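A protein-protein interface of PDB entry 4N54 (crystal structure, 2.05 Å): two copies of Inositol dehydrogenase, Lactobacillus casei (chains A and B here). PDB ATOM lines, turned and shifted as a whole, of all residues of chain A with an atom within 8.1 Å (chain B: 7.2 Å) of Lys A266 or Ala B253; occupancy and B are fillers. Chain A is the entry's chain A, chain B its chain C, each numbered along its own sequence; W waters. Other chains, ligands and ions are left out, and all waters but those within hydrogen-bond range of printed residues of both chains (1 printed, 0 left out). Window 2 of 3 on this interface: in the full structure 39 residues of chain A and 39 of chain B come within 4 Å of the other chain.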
ATOM      1  N   GLY A 154     -10.881   1.917  29.183  1.00  0.00           N
ATOM      2  CA  GLY A 154      -9.864   1.848  28.163  1.00  0.00           C
ATOM      3  C   GLY A 154      -9.609   0.475  27.599  1.00  0.00           C
ATOM      4  O   GLY A 154      -8.653   0.270  26.881  1.00  0.00           O
ATOM      5  N   LYS A 155     -10.481  -0.469  27.904  1.00  0.00           N
ATOM      6  CA  LYS A 155     -10.221  -1.845  27.534  1.00  0.00           C
ATOM      7  C   LYS A 155     -10.227  -2.152  26.040  1.00  0.00           C
ATOM      8  O   LYS A 155      -9.721  -3.178  25.628  1.00  0.00           O
ATOM      9  CB  LYS A 155     -11.100  -2.797  28.328  1.00  0.00           C
ATOM     10  CG  LYS A 155     -10.563  -3.043  29.750  1.00  0.00           C
ATOM     11  CD  LYS A 155      -9.188  -3.719  29.701  1.00  0.00           C
ATOM     12  CE  LYS A 155      -8.680  -4.193  31.068  1.00  0.00           C
ATOM     13  NZ  LYS A 155      -7.459  -5.036  30.947  1.00  0.00           N
ATOM     14  N   ILE A 156     -10.777  -1.254  25.230  1.00  0.00           N
ATOM     15  CA  ILE A 156     -10.685  -1.412  23.785  1.00  0.00           C
ATOM     16  C   ILE A 156     -10.130  -0.181  23.073  1.00  0.00           C
ATOM     17  O   ILE A 156     -10.263  -0.042  21.871  1.00  0.00           O
ATOM     18  CB  ILE A 156     -12.023  -1.841  23.156  1.00  0.00           C
ATOM     19  CG1 ILE A 156     -13.078  -0.770  23.370  1.00  0.00           C
ATOM     20  CG2 ILE A 156     -12.462  -3.170  23.715  1.00  0.00           C
ATOM     21  CD1 ILE A 156     -14.045  -0.666  22.282  1.00  0.00           C
ATOM     22  N   GLY A 157      -9.487   0.697  23.829  1.00  0.00           N
ATOM     23  CA  GLY A 157      -8.963   1.922  23.269  1.00  0.00           C
ATOM     24  C   GLY A 157     -10.054   2.887  22.866  1.00  0.00           C
ATOM     25  O   GLY A 157     -11.107   2.921  23.461  1.00  0.00           O
ATOM     26  N   ASP A 158      -9.788   3.676  21.842  1.00  0.00           N
ATOM     27  CA  ASP A 158     -10.750   4.653  21.379  1.00  0.00           C
ATOM     28  C   ASP A 158     -11.679   4.064  20.329  1.00  0.00           C
ATOM     29  O   ASP A 158     -11.265   3.293  19.494  1.00  0.00           O
ATOM     30  CB  ASP A 158     -10.048   5.874  20.799  1.00  0.00           C
ATOM     31  CG  ASP A 158      -9.229   6.621  21.827  1.00  0.00           C
ATOM     32  OD1 ASP A 158      -9.582   6.603  23.014  1.00  0.00           O
ATOM     33  OD2 ASP A 158      -8.230   7.222  21.435  1.00  0.00           O
ATOM     34  N   ILE A 159     -12.936   4.467  20.392  1.00  0.00           N
ATOM     35  CA  ILE A 159     -13.949   3.979  19.486  1.00  0.00           C
ATOM     36  C   ILE A 159     -13.694   4.435  18.062  1.00  0.00           C
ATOM     37  O   ILE A 159     -13.528   5.606  17.812  1.00  0.00           O
ATOM     38  CB  ILE A 159     -15.345   4.404  19.934  1.00  0.00           C
ATOM     39  CG1 ILE A 159     -15.711   3.738  21.256  1.00  0.00           C
ATOM     40  CG2 ILE A 159     -16.342   4.058  18.881  1.00  0.00           C
ATOM     41  CD1 ILE A 159     -16.835   4.346  21.951  1.00  0.00           C
ATOM     42  N   THR A 160     -13.656   3.479  17.150  1.00  0.00           N
ATOM     43  CA  THR A 160     -13.562   3.737  15.731  1.00  0.00           C
ATOM     44  C   THR A 160     -14.876   3.491  14.991  1.00  0.00           C
ATOM     45  O   THR A 160     -15.163   4.167  14.027  1.00  0.00           O
ATOM     46  CB  THR A 160     -12.473   2.900  15.076  1.00  0.00           C
ATOM     47  OG1 THR A 160     -12.770   1.514  15.226  1.00  0.00           O
ATOM     48  CG2 THR A 160     -11.125   3.198  15.696  1.00  0.00           C
ATOM     49  N   ILE A 263     -16.233  -1.277  17.858  1.00  0.00           N
ATOM     50  CA  ILE A 263     -14.876  -1.502  17.404  1.00  0.00           C
ATOM     51  C   ILE A 263     -13.971  -0.359  17.879  1.00  0.00           C
ATOM     52  O   ILE A 263     -14.336   0.807  17.805  1.00  0.00           O
ATOM     53  CB  ILE A 263     -14.801  -1.646  15.885  1.00  0.00           C
ATOM     54  CG1 ILE A 263     -15.670  -2.808  15.406  1.00  0.00           C
ATOM     55  CG2 ILE A 263     -13.385  -1.832  15.419  1.00  0.00           C
ATOM     56  CD1 ILE A 263     -15.558  -3.035  13.958  1.00  0.00           C
ATOM     57  N   GLY A 264     -12.798  -0.721  18.378  1.00  0.00           N
ATOM     58  CA  GLY A 264     -11.861   0.237  18.915  1.00  0.00           C
ATOM     59  C   GLY A 264     -10.437   0.022  18.466  1.00  0.00           C
ATOM     60  O   GLY A 264     -10.129  -0.918  17.752  1.00  0.00           O
ATOM     61  N   THR A 265      -9.561   0.910  18.907  1.00  0.00           N
ATOM     62  CA  THR A 265      -8.182   0.907  18.471  1.00  0.00           C
ATOM     63  C   THR A 265      -7.377  -0.254  19.029  1.00  0.00           C
ATOM     64  O   THR A 265      -6.359  -0.614  18.482  1.00  0.00           O
ATOM     65  CB  THR A 265      -7.484   2.246  18.818  1.00  0.00           C
ATOM     66  OG1 THR A 265      -7.500   2.457  20.228  1.00  0.00           O
ATOM     67  CG2 THR A 265      -8.190   3.398  18.144  1.00  0.00           C
ATOM     68  N   LYS A 266      -7.854  -0.830  20.123  1.00  0.00           N
ATOM     69  CA  LYS A 266      -7.136  -1.880  20.839  1.00  0.00           C
ATOM     70  C   LYS A 266      -7.969  -3.138  21.000  1.00  0.00           C
ATOM     71  O   LYS A 266      -7.517  -4.119  21.560  1.00  0.00           O
ATOM     72  CB  LYS A 266      -6.745  -1.392  22.224  1.00  0.00           C
ATOM     73  CG  LYS A 266      -5.813  -0.212  22.247  1.00  0.00           C
ATOM     74  CD  LYS A 266      -5.609   0.256  23.672  1.00  0.00           C
ATOM     75  CE  LYS A 266      -4.741   1.498  23.766  1.00  0.00           C
ATOM     76  NZ  LYS A 266      -3.500   1.342  23.006  1.00  0.00           N
ATOM     77  N   GLY A 267      -9.201  -3.088  20.533  1.00  0.00           N
ATOM     78  CA  GLY A 267     -10.081  -4.220  20.652  1.00  0.00           C
ATOM     79  C   GLY A 267     -11.481  -3.966  20.136  1.00  0.00           C
ATOM     80  O   GLY A 267     -11.749  -2.979  19.492  1.00  0.00           O
ATOM     81  N   MET A 268     -12.379  -4.871  20.482  1.00  0.00           N
ATOM     82  CA  MET A 268     -13.706  -4.890  19.918  1.00  0.00           C
ATOM     83  C   MET A 268     -14.616  -5.657  20.851  1.00  0.00           C
ATOM     84  O   MET A 268     -14.201  -6.652  21.422  1.00  0.00           O
ATOM     85  CB  MET A 268     -13.612  -5.567  18.569  1.00  0.00           C
ATOM     86  CG  MET A 268     -14.878  -5.802  17.827  1.00  0.00           C
ATOM     87  SD  MET A 268     -14.498  -6.522  16.237  1.00  0.00           S
ATOM     88  CE  MET A 268     -16.145  -6.822  15.664  1.00  0.00           C
ATOM     89  N   ILE B 167     -10.903  -7.684   7.928  1.00  0.00           N
ATOM     90  CA  ILE B 167      -9.991  -6.887   8.726  1.00  0.00           C
ATOM     91  C   ILE B 167      -8.708  -7.643   9.022  1.00  0.00           C
ATOM     92  O   ILE B 167      -8.723  -8.686   9.655  1.00  0.00           O
ATOM     93  CB  ILE B 167     -10.631  -6.456  10.033  1.00  0.00           C
ATOM     94  CG1 ILE B 167     -11.985  -5.833   9.776  1.00  0.00           C
ATOM     95  CG2 ILE B 167      -9.735  -5.487  10.783  1.00  0.00           C
ATOM     96  CD1 ILE B 167     -12.751  -5.580  10.977  1.00  0.00           C
ATOM     97  N   ASP B 168      -7.603  -7.094   8.538  1.00  0.00           N
ATOM     98  CA  ASP B 168      -6.278  -7.637   8.772  1.00  0.00           C
ATOM     99  C   ASP B 168      -5.846  -7.484  10.231  1.00  0.00           C
ATOM    100  O   ASP B 168      -6.294  -6.593  10.916  1.00  0.00           O
ATOM    101  CB  ASP B 168      -5.271  -6.988   7.832  1.00  0.00           C
ATOM    102  CG  ASP B 168      -4.925  -7.860   6.658  1.00  0.00           C
ATOM    103  OD1 ASP B 168      -5.233  -9.060   6.691  1.00  0.00           O
ATOM    104  OD2 ASP B 168      -4.327  -7.349   5.707  1.00  0.00           O
ATOM    105  N   PRO B 169      -4.996  -8.393  10.706  1.00  0.00           N
ATOM    106  CA  PRO B 169      -4.590  -8.447  12.105  1.00  0.00           C
ATOM    107  C   PRO B 169      -3.596  -7.346  12.478  1.00  0.00           C
ATOM    108  O   PRO B 169      -2.762  -6.956  11.682  1.00  0.00           O
ATOM    109  CB  PRO B 169      -3.943  -9.811  12.206  1.00  0.00           C
ATOM    110  CG  PRO B 169      -3.408 -10.034  10.900  1.00  0.00           C
ATOM    111  CD  PRO B 169      -4.367  -9.471   9.940  1.00  0.00           C
ATOM    112  N   ALA B 170      -3.727  -6.850  13.693  1.00  0.00           N
ATOM    113  CA  ALA B 170      -2.952  -5.720  14.153  1.00  0.00           C
ATOM    114  C   ALA B 170      -1.468  -6.044  14.192  1.00  0.00           C
ATOM    115  O   ALA B 170      -0.644  -5.153  14.136  1.00  0.00           O
ATOM    116  CB  ALA B 170      -3.440  -5.269  15.491  1.00  0.00           C
ATOM    117  N   ALA B 171      -1.141  -7.326  14.258  1.00  0.00           N
ATOM    118  CA  ALA B 171       0.242  -7.755  14.216  1.00  0.00           C
ATOM    119  C   ALA B 171       0.906  -7.365  12.906  1.00  0.00           C
ATOM    120  O   ALA B 171       2.118  -7.318  12.814  1.00  0.00           O
ATOM    121  CB  ALA B 171       0.356  -9.244  14.446  1.00  0.00           C
ATOM    122  N   ALA B 219      -6.083   4.794  15.315  1.00  0.00           N
ATOM    123  CA  ALA B 219      -5.031   4.086  16.001  1.00  0.00           C
ATOM    124  C   ALA B 219      -3.690   4.617  15.542  1.00  0.00           C
ATOM    125  O   ALA B 219      -2.802   4.818  16.338  1.00  0.00           O
ATOM    126  CB  ALA B 219      -5.118   2.613  15.720  1.00  0.00           C
ATOM    127  N   ARG B 250      -7.278  -3.005   8.907  1.00  0.00           N
ATOM    128  CA  ARG B 250      -5.908  -3.462   8.996  1.00  0.00           C
ATOM    129  C   ARG B 250      -5.479  -3.599  10.441  1.00  0.00           C
ATOM    130  O   ARG B 250      -4.369  -4.002  10.720  1.00  0.00           O
ATOM    131  CB  ARG B 250      -4.980  -2.482   8.284  1.00  0.00           C
ATOM    132  CG  ARG B 250      -5.213  -2.336   6.813  1.00  0.00           C
ATOM    133  CD  ARG B 250      -4.195  -1.387   6.214  1.00  0.00           C
ATOM    134  NE  ARG B 250      -4.641  -0.750   4.981  1.00  0.00           N
ATOM    135  CZ  ARG B 250      -4.524  -1.290   3.783  1.00  0.00           C
ATOM    136  NH1 ARG B 250      -3.994  -2.485   3.641  1.00  0.00           N
ATOM    137  NH2 ARG B 250      -4.945  -0.636   2.725  1.00  0.00           N
ATOM    138  N   ASN B 251      -6.387  -3.277  11.346  1.00  0.00           N
ATOM    139  CA  ASN B 251      -6.094  -3.241  12.770  1.00  0.00           C
ATOM    140  C   ASN B 251      -7.018  -4.088  13.669  1.00  0.00           C
ATOM    141  O   ASN B 251      -7.577  -3.586  14.623  1.00  0.00           O
ATOM    142  CB  ASN B 251      -6.105  -1.798  13.236  1.00  0.00           C
ATOM    143  CG  ASN B 251      -5.479  -1.618  14.575  1.00  0.00           C
ATOM    144  OD1 ASN B 251      -4.574  -2.343  14.937  1.00  0.00           O
ATOM    145  ND2 ASN B 251      -5.969  -0.659  15.328  1.00  0.00           N
ATOM    146  N   ALA B 252      -7.172  -5.368  13.366  1.00  0.00           N
ATOM    147  CA  ALA B 252      -7.961  -6.241  14.236  1.00  0.00           C
ATOM    148  C   ALA B 252      -7.113  -6.810  15.366  1.00  0.00           C
ATOM    149  O   ALA B 252      -6.186  -7.554  15.137  1.00  0.00           O
ATOM    150  CB  ALA B 252      -8.635  -7.350  13.454  1.00  0.00           C
ATOM    151  N   ALA B 253      -7.462  -6.442  16.587  1.00  0.00           N
ATOM    152  CA  ALA B 253      -6.728  -6.845  17.769  1.00  0.00           C
ATOM    153  C   ALA B 253      -6.733  -8.341  18.010  1.00  0.00           C
ATOM    154  O   ALA B 253      -5.765  -8.878  18.509  1.00  0.00           O
ATOM    155  CB  ALA B 253      -7.240  -6.122  18.963  1.00  0.00           C
ATOM    156  N   HIS B 254      -7.813  -9.014  17.636  1.00  0.00           N
ATOM    157  CA  HIS B 254      -7.947 -10.435  17.929  1.00  0.00           C
ATOM    158  C   HIS B 254      -7.350 -11.369  16.893  1.00  0.00           C
ATOM    159  O   HIS B 254      -7.049 -12.511  17.196  1.00  0.00           O
ATOM    160  CB  HIS B 254      -9.398 -10.820  18.228  1.00  0.00           C
ATOM    161  CG  HIS B 254     -10.360 -10.474  17.142  1.00  0.00           C
ATOM    162  ND1 HIS B 254     -10.738  -9.183  16.870  1.00  0.00           N
ATOM    163  CD2 HIS B 254     -11.045 -11.253  16.283  1.00  0.00           C
ATOM    164  CE1 HIS B 254     -11.605  -9.182  15.878  1.00  0.00           C
ATOM    165  NE2 HIS B 254     -11.807 -10.428  15.506  1.00  0.00           N
ATOM    166  N   GLY B 255      -7.178 -10.882  15.676  1.00  0.00           N
ATOM    167  CA  GLY B 255      -6.595 -11.685  14.636  1.00  0.00           C
ATOM    168  C   GLY B 255      -7.052 -11.290  13.262  1.00  0.00           C
ATOM    169  O   GLY B 255      -7.150 -10.120  12.954  1.00  0.00           O
ATOM    170  N   TYR B 256      -7.332 -12.284  12.434  1.00  0.00           N
ATOM    171  CA  TYR B 256      -7.811 -12.068  11.081  1.00  0.00           C
ATOM    172  C   TYR B 256      -9.314 -12.252  11.045  1.00  0.00           C
ATOM    173  O   TYR B 256      -9.815 -13.354  11.082  1.00  0.00           O
ATOM    174  CB  TYR B 256      -7.124 -13.042  10.152  1.00  0.00           C
ATOM    175  CG  TYR B 256      -7.451 -12.913   8.687  1.00  0.00           C
ATOM    176  CD1 TYR B 256      -7.432 -11.686   8.049  1.00  0.00           C
ATOM    177  CD2 TYR B 256      -7.730 -14.025   7.932  1.00  0.00           C
ATOM    178  CE1 TYR B 256      -7.710 -11.586   6.718  1.00  0.00           C
ATOM    179  CE2 TYR B 256      -8.010 -13.933   6.611  1.00  0.00           C
ATOM    180  CZ  TYR B 256      -7.995 -12.717   6.001  1.00  0.00           C
ATOM    181  OH  TYR B 256      -8.272 -12.638   4.672  1.00  0.00           O
ATOM    182  N   THR B 292      -8.022 -17.684  18.063  1.00  0.00           N
ATOM    183  CA  THR B 292      -8.467 -17.244  16.763  1.00  0.00           C
ATOM    184  C   THR B 292      -7.460 -17.500  15.671  1.00  0.00           C
ATOM    185  O   THR B 292      -6.289 -17.692  15.937  1.00  0.00           O
ATOM    186  CB  THR B 292      -8.744 -15.742  16.755  1.00  0.00           C
ATOM    187  OG1 THR B 292      -7.587 -15.045  17.210  1.00  0.00           O
ATOM    188  CG2 THR B 292      -9.898 -15.407  17.635  1.00  0.00           C
ATOM    189  N   GLN B 294      -5.168 -16.184  12.610  1.00  0.00           N
ATOM    190  CA  GLN B 294      -4.300 -15.026  12.704  1.00  0.00           C
ATOM    191  C   GLN B 294      -3.985 -14.354  11.383  1.00  0.00           C
ATOM    192  O   GLN B 294      -3.575 -13.212  11.366  1.00  0.00           O
ATOM    193  CB  GLN B 294      -3.000 -15.424  13.386  1.00  0.00           C
ATOM    194  CG  GLN B 294      -3.151 -15.778  14.830  1.00  0.00           C
ATOM    195  CD  GLN B 294      -3.481 -14.601  15.674  1.00  0.00           C
ATOM    196  OE1 GLN B 294      -2.711 -13.665  15.766  1.00  0.00           O
ATOM    197  NE2 GLN B 294      -4.627 -14.637  16.304  1.00  0.00           N
HETATM  198  O   HOH W   1      -5.740  -3.520  17.594  1.00  0.00           O
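The backbone carbonyl oxygen (O) of Thr A265 lies within hydrogen-bond range of the side-chain amide nitrogen (ND2) of Asn B251, 3.2 Å away.
The backbone NH of Thr A265 sits at hydrogen-bond distance from the backbone carbonyl oxygen of Ile A156, at 3.2 Å.
N of Lys A266 is in hydrogen-bond range of O of Ile A156 (3.1 Å).
The backbone NH (N) of Gly A267 sits at hydrogen-bond distance from the backbone carbonyl oxygen (O) of Ile A156 (3.5 Å).
The backbone carbonyl oxygen (O) of Asp A158 sits at hydrogen-bond distance from the backbone NH (N) of Thr A265 (3.0 Å).
O of Asp B168 lies within hydrogen-bond range of N of Asn B251.
OG1 of Thr B292 lies within hydrogen-bond range of O of His B254 (2.6 Å).
Among the printed residues, merely in contact across the chains: Thr A265 with Ala B219, Lys A266 with Ala B253, Gly A267 with Ala B253 and Met A268 with His B254.
Printed residues of chain B within 4 Å of Thr A265: Ala B219 and Asn B251.
Lys A266 touches just one residue of chain B: Ala B253.
Printed residues of chain A within 4 Å of Ala B219: Thr A265.
Arg B250 touches none of the printed residues of chain A.
Of the printed residues of chain A, Asn B251 touches Thr A265 (3.2 Å).
Of chain A, only Lys A266 (3.3 Å) and Gly A267 (3.8 Å) come within 4 Å of Ala B253.
Of the printed residues of chain A, His B254 touches Met A268 (3.9 Å).
Hydrophobic or aromatic side chains of chain B within 4 Å of the printed part of chain A: Ala B219, Ala B253 and His B254.
Of the 13 printed residues of chain A, 4 touch a printed residue of chain B.
Among the printed residues, 5 pairs touch across the chains.
Among the printed residues, no Asp or Glu carboxylate lies within 4 Å of a Lys or Arg side-chain nitrogen of the other chain.
No position is printed for both chains.
Of the 5 pairs that touch across the chains among the printed residues, none has its exchanged pair printed and touching as well.
Water W1 lies within hydrogen-bond range of the backbone carbonyl oxygen of Thr A265 (3.1 Å) and the side-chain amide oxygen of Asn B251 (3.1 Å).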
